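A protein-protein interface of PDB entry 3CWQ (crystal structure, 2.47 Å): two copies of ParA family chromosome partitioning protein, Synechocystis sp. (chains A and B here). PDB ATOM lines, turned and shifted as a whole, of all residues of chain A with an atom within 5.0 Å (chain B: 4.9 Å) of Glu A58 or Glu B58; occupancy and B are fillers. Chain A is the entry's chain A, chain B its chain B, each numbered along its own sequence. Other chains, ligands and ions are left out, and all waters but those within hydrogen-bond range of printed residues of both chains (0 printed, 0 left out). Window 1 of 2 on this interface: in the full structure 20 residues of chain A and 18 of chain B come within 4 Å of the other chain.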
ATOM      1  N   ILE A  34     -28.237 -36.727 -17.042  1.00  0.00           N
ATOM      2  CA  ILE A  34     -27.426 -35.922 -17.896  1.00  0.00           C
ATOM      3  C   ILE A  34     -27.129 -34.695 -17.149  1.00  0.00           C
ATOM      4  O   ILE A  34     -28.020 -33.934 -16.883  1.00  0.00           O
ATOM      5  CB  ILE A  34     -28.205 -35.454 -19.186  1.00  0.00           C
ATOM      6  CG1 ILE A  34     -28.445 -36.607 -20.121  1.00  0.00           C
ATOM      7  CG2 ILE A  34     -27.404 -34.440 -19.909  1.00  0.00           C
ATOM      8  CD1 ILE A  34     -29.678 -36.440 -21.098  1.00  0.00           C
ATOM      9  N   ASP A  35     -25.874 -34.436 -16.890  1.00  0.00           N
ATOM     10  CA  ASP A  35     -25.523 -33.268 -16.051  1.00  0.00           C
ATOM     11  C   ASP A  35     -25.355 -32.046 -16.950  1.00  0.00           C
ATOM     12  O   ASP A  35     -24.427 -32.001 -17.702  1.00  0.00           O
ATOM     13  CB  ASP A  35     -24.195 -33.563 -15.302  1.00  0.00           C
ATOM     14  CG  ASP A  35     -23.837 -32.468 -14.323  1.00  0.00           C
ATOM     15  OD1 ASP A  35     -22.941 -32.704 -13.381  1.00  0.00           O
ATOM     16  OD2 ASP A  35     -24.400 -31.322 -14.461  1.00  0.00           O
ATOM     17  N   GLY A  36     -26.250 -31.063 -16.931  1.00  0.00           N
ATOM     18  CA  GLY A  36     -25.981 -29.828 -17.689  1.00  0.00           C
ATOM     19  C   GLY A  36     -25.783 -28.596 -16.813  1.00  0.00           C
ATOM     20  O   GLY A  36     -26.215 -27.488 -17.175  1.00  0.00           O
ATOM     21  N   ARG A  40     -21.174 -28.991 -12.574  1.00  0.00           N
ATOM     22  CA  ARG A  40     -20.978 -30.414 -12.813  1.00  0.00           C
ATOM     23  C   ARG A  40     -20.920 -31.111 -11.407  1.00  0.00           C
ATOM     24  O   ARG A  40     -20.151 -32.076 -11.159  1.00  0.00           O
ATOM     25  CB  ARG A  40     -19.635 -30.623 -13.545  1.00  0.00           C
ATOM     26  CG  ARG A  40     -19.679 -30.922 -14.994  1.00  0.00           C
ATOM     27  CD  ARG A  40     -20.720 -30.197 -15.826  1.00  0.00           C
ATOM     28  NE  ARG A  40     -20.663 -30.492 -17.285  1.00  0.00           N
ATOM     29  CZ  ARG A  40     -21.327 -29.760 -18.244  1.00  0.00           C
ATOM     30  NH1 ARG A  40     -21.216 -30.079 -19.540  1.00  0.00           N
ATOM     31  NH2 ARG A  40     -22.080 -28.702 -17.922  1.00  0.00           N
ATOM     32  N   VAL A  56     -23.687 -38.857 -17.176  1.00  0.00           N
ATOM     33  CA  VAL A  56     -22.871 -38.413 -18.251  1.00  0.00           C
ATOM     34  C   VAL A  56     -22.898 -36.870 -18.309  1.00  0.00           C
ATOM     35  O   VAL A  56     -23.652 -36.249 -17.604  1.00  0.00           O
ATOM     36  CB  VAL A  56     -23.369 -39.067 -19.557  1.00  0.00           C
ATOM     37  CG1 VAL A  56     -23.469 -40.543 -19.316  1.00  0.00           C
ATOM     38  CG2 VAL A  56     -24.812 -38.525 -20.018  1.00  0.00           C
ATOM     39  N   ASP A  57     -22.118 -36.238 -19.172  1.00  0.00           N
ATOM     40  CA  ASP A  57     -22.033 -34.798 -19.276  1.00  0.00           C
ATOM     41  C   ASP A  57     -23.002 -34.402 -20.353  1.00  0.00           C
ATOM     42  O   ASP A  57     -23.321 -35.190 -21.222  1.00  0.00           O
ATOM     43  CB  ASP A  57     -20.626 -34.462 -19.719  1.00  0.00           C
ATOM     44  CG  ASP A  57     -20.385 -33.007 -19.785  1.00  0.00           C
ATOM     45  OD1 ASP A  57     -20.846 -32.414 -20.800  1.00  0.00           O
ATOM     46  OD2 ASP A  57     -19.763 -32.395 -18.861  1.00  0.00           O
ATOM     47  N   GLU A  58     -23.528 -33.195 -20.325  1.00  0.00           N
ATOM     48  CA  GLU A  58     -24.483 -32.827 -21.397  1.00  0.00           C
ATOM     49  C   GLU A  58     -23.967 -32.862 -22.845  1.00  0.00           C
ATOM     50  O   GLU A  58     -24.770 -32.909 -23.792  1.00  0.00           O
ATOM     51  CB  GLU A  58     -25.060 -31.479 -21.082  1.00  0.00           C
ATOM     52  CG  GLU A  58     -24.864 -30.452 -22.159  1.00  0.00           C
ATOM     53  CD  GLU A  58     -24.797 -29.055 -21.577  1.00  0.00           C
ATOM     54  OE1 GLU A  58     -23.834 -28.795 -20.748  1.00  0.00           O
ATOM     55  OE2 GLU A  58     -25.716 -28.240 -21.935  1.00  0.00           O
ATOM     56  N   ARG A  59     -22.654 -32.792 -23.039  1.00  0.00           N
ATOM     57  CA  ARG A  59     -22.059 -32.940 -24.380  1.00  0.00           C
ATOM     58  C   ARG A  59     -22.256 -34.353 -24.891  1.00  0.00           C
ATOM     59  O   ARG A  59     -22.136 -34.568 -26.090  1.00  0.00           O
ATOM     60  CB  ARG A  59     -20.530 -32.672 -24.390  1.00  0.00           C
ATOM     61  CG  ARG A  59     -20.096 -31.338 -23.783  1.00  0.00           C
ATOM     62  CD  ARG A  59     -20.865 -30.170 -24.356  1.00  0.00           C
ATOM     63  NE  ARG A  59     -19.981 -29.027 -24.316  1.00  0.00           N
ATOM     64  CZ  ARG A  59     -20.152 -27.874 -24.961  1.00  0.00           C
ATOM     65  NH1 ARG A  59     -21.248 -27.616 -25.721  1.00  0.00           N
ATOM     66  NH2 ARG A  59     -19.181 -26.964 -24.840  1.00  0.00           N
ATOM     67  N   GLN A  60     -22.521 -35.296 -23.967  1.00  0.00           N
ATOM     68  CA  GLN A  60     -22.778 -36.715 -24.282  1.00  0.00           C
ATOM     69  C   GLN A  60     -24.277 -37.149 -24.312  1.00  0.00           C
ATOM     70  O   GLN A  60     -24.627 -38.309 -24.505  1.00  0.00           O
ATOM     71  CB  GLN A  60     -21.945 -37.656 -23.391  1.00  0.00           C
ATOM     72  CG  GLN A  60     -20.447 -37.464 -23.530  1.00  0.00           C
ATOM     73  CD  GLN A  60     -19.737 -37.350 -22.173  1.00  0.00           C
ATOM     74  OE1 GLN A  60     -20.179 -37.941 -21.185  1.00  0.00           O
ATOM     75  NE2 GLN A  60     -18.641 -36.567 -22.126  1.00  0.00           N
ATOM     76  N   ALA A  61     -25.152 -36.194 -24.160  1.00  0.00           N
ATOM     77  CA  ALA A  61     -26.571 -36.477 -24.235  1.00  0.00           C
ATOM     78  C   ALA A  61     -26.984 -37.117 -25.514  1.00  0.00           C
ATOM     79  O   ALA A  61     -27.667 -38.100 -25.429  1.00  0.00           O
ATOM     80  CB  ALA A  61     -27.411 -35.221 -23.917  1.00  0.00           C
ATOM     81  N   ARG A  78     -31.319 -20.544 -17.422  1.00  0.00           N
ATOM     82  CA  ARG A  78     -30.622 -19.689 -18.445  1.00  0.00           C
ATOM     83  C   ARG A  78     -31.456 -18.942 -19.547  1.00  0.00           C
ATOM     84  O   ARG A  78     -31.654 -19.499 -20.624  1.00  0.00           O
ATOM     85  CB  ARG A  78     -29.351 -20.404 -19.059  1.00  0.00           C
ATOM     86  CG  ARG A  78     -29.432 -21.491 -20.138  1.00  0.00           C
ATOM     87  CD  ARG A  78     -28.416 -22.641 -19.812  1.00  0.00           C
ATOM     88  NE  ARG A  78     -27.830 -23.425 -20.927  1.00  0.00           N
ATOM     89  CZ  ARG A  78     -27.047 -24.529 -20.745  1.00  0.00           C
ATOM     90  NH1 ARG A  78     -26.795 -24.956 -19.500  1.00  0.00           N
ATOM     91  NH2 ARG A  78     -26.505 -25.209 -21.777  1.00  0.00           N
ATOM     92  N   ILE B  34     -28.865 -30.627 -33.930  1.00  0.00           N
ATOM     93  CA  ILE B  34     -28.976 -30.016 -32.581  1.00  0.00           C
ATOM     94  C   ILE B  34     -28.171 -28.650 -32.305  1.00  0.00           C
ATOM     95  O   ILE B  34     -26.930 -28.528 -32.447  1.00  0.00           O
ATOM     96  CB  ILE B  34     -28.502 -31.071 -31.500  1.00  0.00           C
ATOM     97  CG1 ILE B  34     -29.294 -32.392 -31.539  1.00  0.00           C
ATOM     98  CG2 ILE B  34     -28.468 -30.454 -30.145  1.00  0.00           C
ATOM     99  CD1 ILE B  34     -28.391 -33.505 -30.981  1.00  0.00           C
ATOM    100  N   ASP B  35     -28.885 -27.683 -31.749  1.00  0.00           N
ATOM    101  CA  ASP B  35     -28.464 -26.256 -31.685  1.00  0.00           C
ATOM    102  C   ASP B  35     -28.077 -25.952 -30.240  1.00  0.00           C
ATOM    103  O   ASP B  35     -28.928 -25.848 -29.378  1.00  0.00           O
ATOM    104  CB  ASP B  35     -29.619 -25.395 -32.195  1.00  0.00           C
ATOM    105  CG  ASP B  35     -29.224 -24.002 -32.440  1.00  0.00           C
ATOM    106  OD1 ASP B  35     -30.043 -23.160 -33.049  1.00  0.00           O
ATOM    107  OD2 ASP B  35     -28.128 -23.639 -32.009  1.00  0.00           O
ATOM    108  N   GLY B  36     -26.782 -25.824 -29.968  1.00  0.00           N
ATOM    109  CA  GLY B  36     -26.267 -25.575 -28.595  1.00  0.00           C
ATOM    110  C   GLY B  36     -25.535 -24.270 -28.627  1.00  0.00           C
ATOM    111  O   GLY B  36     -24.632 -24.026 -27.828  1.00  0.00           O
ATOM    112  N   ARG B  40     -28.617 -19.451 -30.957  1.00  0.00           N
ATOM    113  CA  ARG B  40     -29.588 -20.136 -31.791  1.00  0.00           C
ATOM    114  C   ARG B  40     -29.670 -19.738 -33.289  1.00  0.00           C
ATOM    115  O   ARG B  40     -30.722 -19.885 -33.890  1.00  0.00           O
ATOM    116  CB  ARG B  40     -30.976 -20.002 -31.174  1.00  0.00           C
ATOM    117  CG  ARG B  40     -31.061 -20.662 -29.832  1.00  0.00           C
ATOM    118  CD  ARG B  40     -30.494 -22.089 -29.812  1.00  0.00           C
ATOM    119  NE  ARG B  40     -30.915 -22.773 -28.626  1.00  0.00           N
ATOM    120  CZ  ARG B  40     -30.105 -23.109 -27.627  1.00  0.00           C
ATOM    121  NH1 ARG B  40     -30.547 -23.729 -26.548  1.00  0.00           N
ATOM    122  NH2 ARG B  40     -28.852 -22.875 -27.722  1.00  0.00           N
ATOM    123  N   VAL B  56     -33.401 -29.029 -33.828  1.00  0.00           N
ATOM    124  CA  VAL B  56     -33.932 -28.909 -32.501  1.00  0.00           C
ATOM    125  C   VAL B  56     -32.916 -28.291 -31.531  1.00  0.00           C
ATOM    126  O   VAL B  56     -31.726 -28.127 -31.816  1.00  0.00           O
ATOM    127  CB  VAL B  56     -34.312 -30.296 -31.878  1.00  0.00           C
ATOM    128  CG1 VAL B  56     -35.376 -31.033 -32.658  1.00  0.00           C
ATOM    129  CG2 VAL B  56     -33.101 -31.137 -31.705  1.00  0.00           C
ATOM    130  N   ASP B  57     -33.382 -27.985 -30.350  1.00  0.00           N
ATOM    131  CA  ASP B  57     -32.639 -27.207 -29.478  1.00  0.00           C
ATOM    132  C   ASP B  57     -31.863 -28.198 -28.675  1.00  0.00           C
ATOM    133  O   ASP B  57     -32.322 -29.297 -28.404  1.00  0.00           O
ATOM    134  CB  ASP B  57     -33.667 -26.536 -28.590  1.00  0.00           C
ATOM    135  CG  ASP B  57     -33.096 -25.478 -27.742  1.00  0.00           C
ATOM    136  OD1 ASP B  57     -32.453 -25.818 -26.740  1.00  0.00           O
ATOM    137  OD2 ASP B  57     -33.228 -24.269 -28.040  1.00  0.00           O
ATOM    138  N   GLU B  58     -30.723 -27.793 -28.239  1.00  0.00           N
ATOM    139  CA  GLU B  58     -29.915 -28.584 -27.377  1.00  0.00           C
ATOM    140  C   GLU B  58     -30.731 -29.176 -26.256  1.00  0.00           C
ATOM    141  O   GLU B  58     -30.383 -30.249 -25.735  1.00  0.00           O
ATOM    142  CB  GLU B  58     -28.873 -27.677 -26.790  1.00  0.00           C
ATOM    143  CG  GLU B  58     -28.071 -28.317 -25.693  1.00  0.00           C
ATOM    144  CD  GLU B  58     -27.220 -27.247 -25.002  1.00  0.00           C
ATOM    145  OE1 GLU B  58     -27.806 -26.184 -24.663  1.00  0.00           O
ATOM    146  OE2 GLU B  58     -25.969 -27.442 -24.878  1.00  0.00           O
ATOM    147  N   ARG B  59     -31.809 -28.503 -25.843  1.00  0.00           N
ATOM    148  CA  ARG B  59     -32.571 -28.994 -24.666  1.00  0.00           C
ATOM    149  C   ARG B  59     -33.392 -30.187 -25.051  1.00  0.00           C
ATOM    150  O   ARG B  59     -34.078 -30.735 -24.192  1.00  0.00           O
ATOM    151  CB  ARG B  59     -33.549 -27.910 -24.177  1.00  0.00           C
ATOM    152  CG  ARG B  59     -33.117 -27.009 -22.993  1.00  0.00           C
ATOM    153  CD  ARG B  59     -31.872 -26.230 -23.139  1.00  0.00           C
ATOM    154  NE  ARG B  59     -31.809 -25.291 -22.052  1.00  0.00           N
ATOM    155  CZ  ARG B  59     -31.139 -25.471 -20.916  1.00  0.00           C
ATOM    156  NH1 ARG B  59     -30.429 -26.574 -20.752  1.00  0.00           N
ATOM    157  NH2 ARG B  59     -31.198 -24.532 -19.942  1.00  0.00           N
ATOM    158  N   GLN B  60     -33.383 -30.563 -26.368  1.00  0.00           N
ATOM    159  CA  GLN B  60     -34.339 -31.511 -26.936  1.00  0.00           C
ATOM    160  C   GLN B  60     -33.489 -32.578 -27.469  1.00  0.00           C
ATOM    161  O   GLN B  60     -33.894 -33.486 -28.207  1.00  0.00           O
ATOM    162  CB  GLN B  60     -35.163 -30.850 -28.036  1.00  0.00           C
ATOM    163  CG  GLN B  60     -35.753 -29.500 -27.659  1.00  0.00           C
ATOM    164  CD  GLN B  60     -36.697 -28.842 -28.800  1.00  0.00           C
ATOM    165  OE1 GLN B  60     -36.244 -28.167 -29.713  1.00  0.00           O
ATOM    166  NE2 GLN B  60     -37.952 -28.950 -28.626  1.00  0.00           N
ATOM    167  N   ALA B  61     -32.269 -32.576 -26.986  1.00  0.00           N
ATOM    168  CA  ALA B  61     -31.265 -33.474 -27.622  1.00  0.00           C
ATOM    169  C   ALA B  61     -31.595 -34.863 -27.159  1.00  0.00           C
ATOM    170  O   ALA B  61     -31.710 -35.769 -27.979  1.00  0.00           O
ATOM    171  CB  ALA B  61     -29.792 -33.019 -27.313  1.00  0.00           C
ATOM    172  N   ARG B  78     -16.531 -24.438 -24.827  1.00  0.00           N
ATOM    173  CA  ARG B  78     -16.536 -23.789 -23.480  1.00  0.00           C
ATOM    174  C   ARG B  78     -15.196 -23.793 -22.711  1.00  0.00           C
ATOM    175  O   ARG B  78     -14.232 -23.104 -23.088  1.00  0.00           O
ATOM    176  CB  ARG B  78     -17.607 -24.443 -22.591  1.00  0.00           C
ATOM    177  CG  ARG B  78     -19.057 -24.320 -23.094  1.00  0.00           C
ATOM    178  CD  ARG B  78     -20.169 -24.889 -22.128  1.00  0.00           C
ATOM    179  NE  ARG B  78     -21.494 -24.549 -22.708  1.00  0.00           N
ATOM    180  CZ  ARG B  78     -22.480 -25.404 -23.080  1.00  0.00           C
ATOM    181  NH1 ARG B  78     -22.394 -26.728 -22.912  1.00  0.00           N
ATOM    182  NH2 ARG B  78     -23.594 -24.906 -23.598  1.00  0.00           N
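Glu B58 touches its own counterpart, Glu A58. Glu A58 touches Arg B78, and with the chains exchanged Arg A78 touches Glu B58. Arg A59 touches Arg B78, and with the chains exchanged Arg A78 touches Arg B59. Arg A78 touches its own counterpart, Arg B78. Of the 6 pairs that touch across the chains among the printed residues, 6 have their exchanged pair printed and touching as well.
Of chain B, only Glu B58 (3.1 Å) and Arg B78 (3.3 Å) come within 4 Å of Glu A58. Of the printed residues of chain A, Arg B78 touches Glu A58 (3.3 Å), Arg A59 (3.2 Å) and Arg A78 (3.4 Å). Printed residues of chain A within 4 Å of Arg B59: Arg A78. Ile B34 touches none of the printed residues of chain A. The nearest printed residue of chain B that does not touch Arg A78 is Arg B40 (6.3 Å).
Printed residues of chain A that touch a printed residue of chain B: Glu A58, Arg A59 and Arg A78. Along chain A the printed residues that touch a printed residue of chain B span positions 58 to 78. Among the printed residues, Asp or Glu carboxylates within 4 Å of a Lys or Arg side-chain nitrogen of the other chain: Glu A58 with Arg B78 (3.3 Å) and Arg A78 with Glu B58 (3.3 Å).
The side-chain carboxylate (OE1) of Glu A58 lies within salt-bridge range of the guanidinium group (NH1) of Arg B78 (3.3 Å). NH2 of Arg A78 lies within salt-bridge range of OE1 of Glu B58, 3.3 Å away. The side-chain carboxylate (OE2) of Glu B58 sits close to the side-chain carboxylate (OE2) of Glu A58, 3.1 Å away. The guanidinium group of Arg B78 lies close to the guanidinium group of Arg A59. NH2 of Arg A78 lies close to NH2 of Arg B78, at 3.4 Å.
The backbone NH (N) of Glu A58 lies within hydrogen-bond range of the backbone carbonyl oxygen (O) of Asp A35 (3.0 Å). The backbone carbonyl oxygen (O) of Gly A36 is in hydrogen-bond range of the guanidinium group (NH1) of Arg A78, 3.5 Å away. NH1 of Arg A40 is in salt-bridge range of OE1 of Glu A58. OE2 of Glu A58 lies within salt-bridge range of NH2 of Arg A78 (3.1 Å). The backbone carbonyl oxygen (O) of Asp B35 sits at hydrogen-bond distance from the backbone NH (N) of Glu B58 (2.9 Å). OD1 of Asp B57 lies close to N of Arg B59.
Among the printed residues, merely in contact across the chains: Arg A78 with Arg B59.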
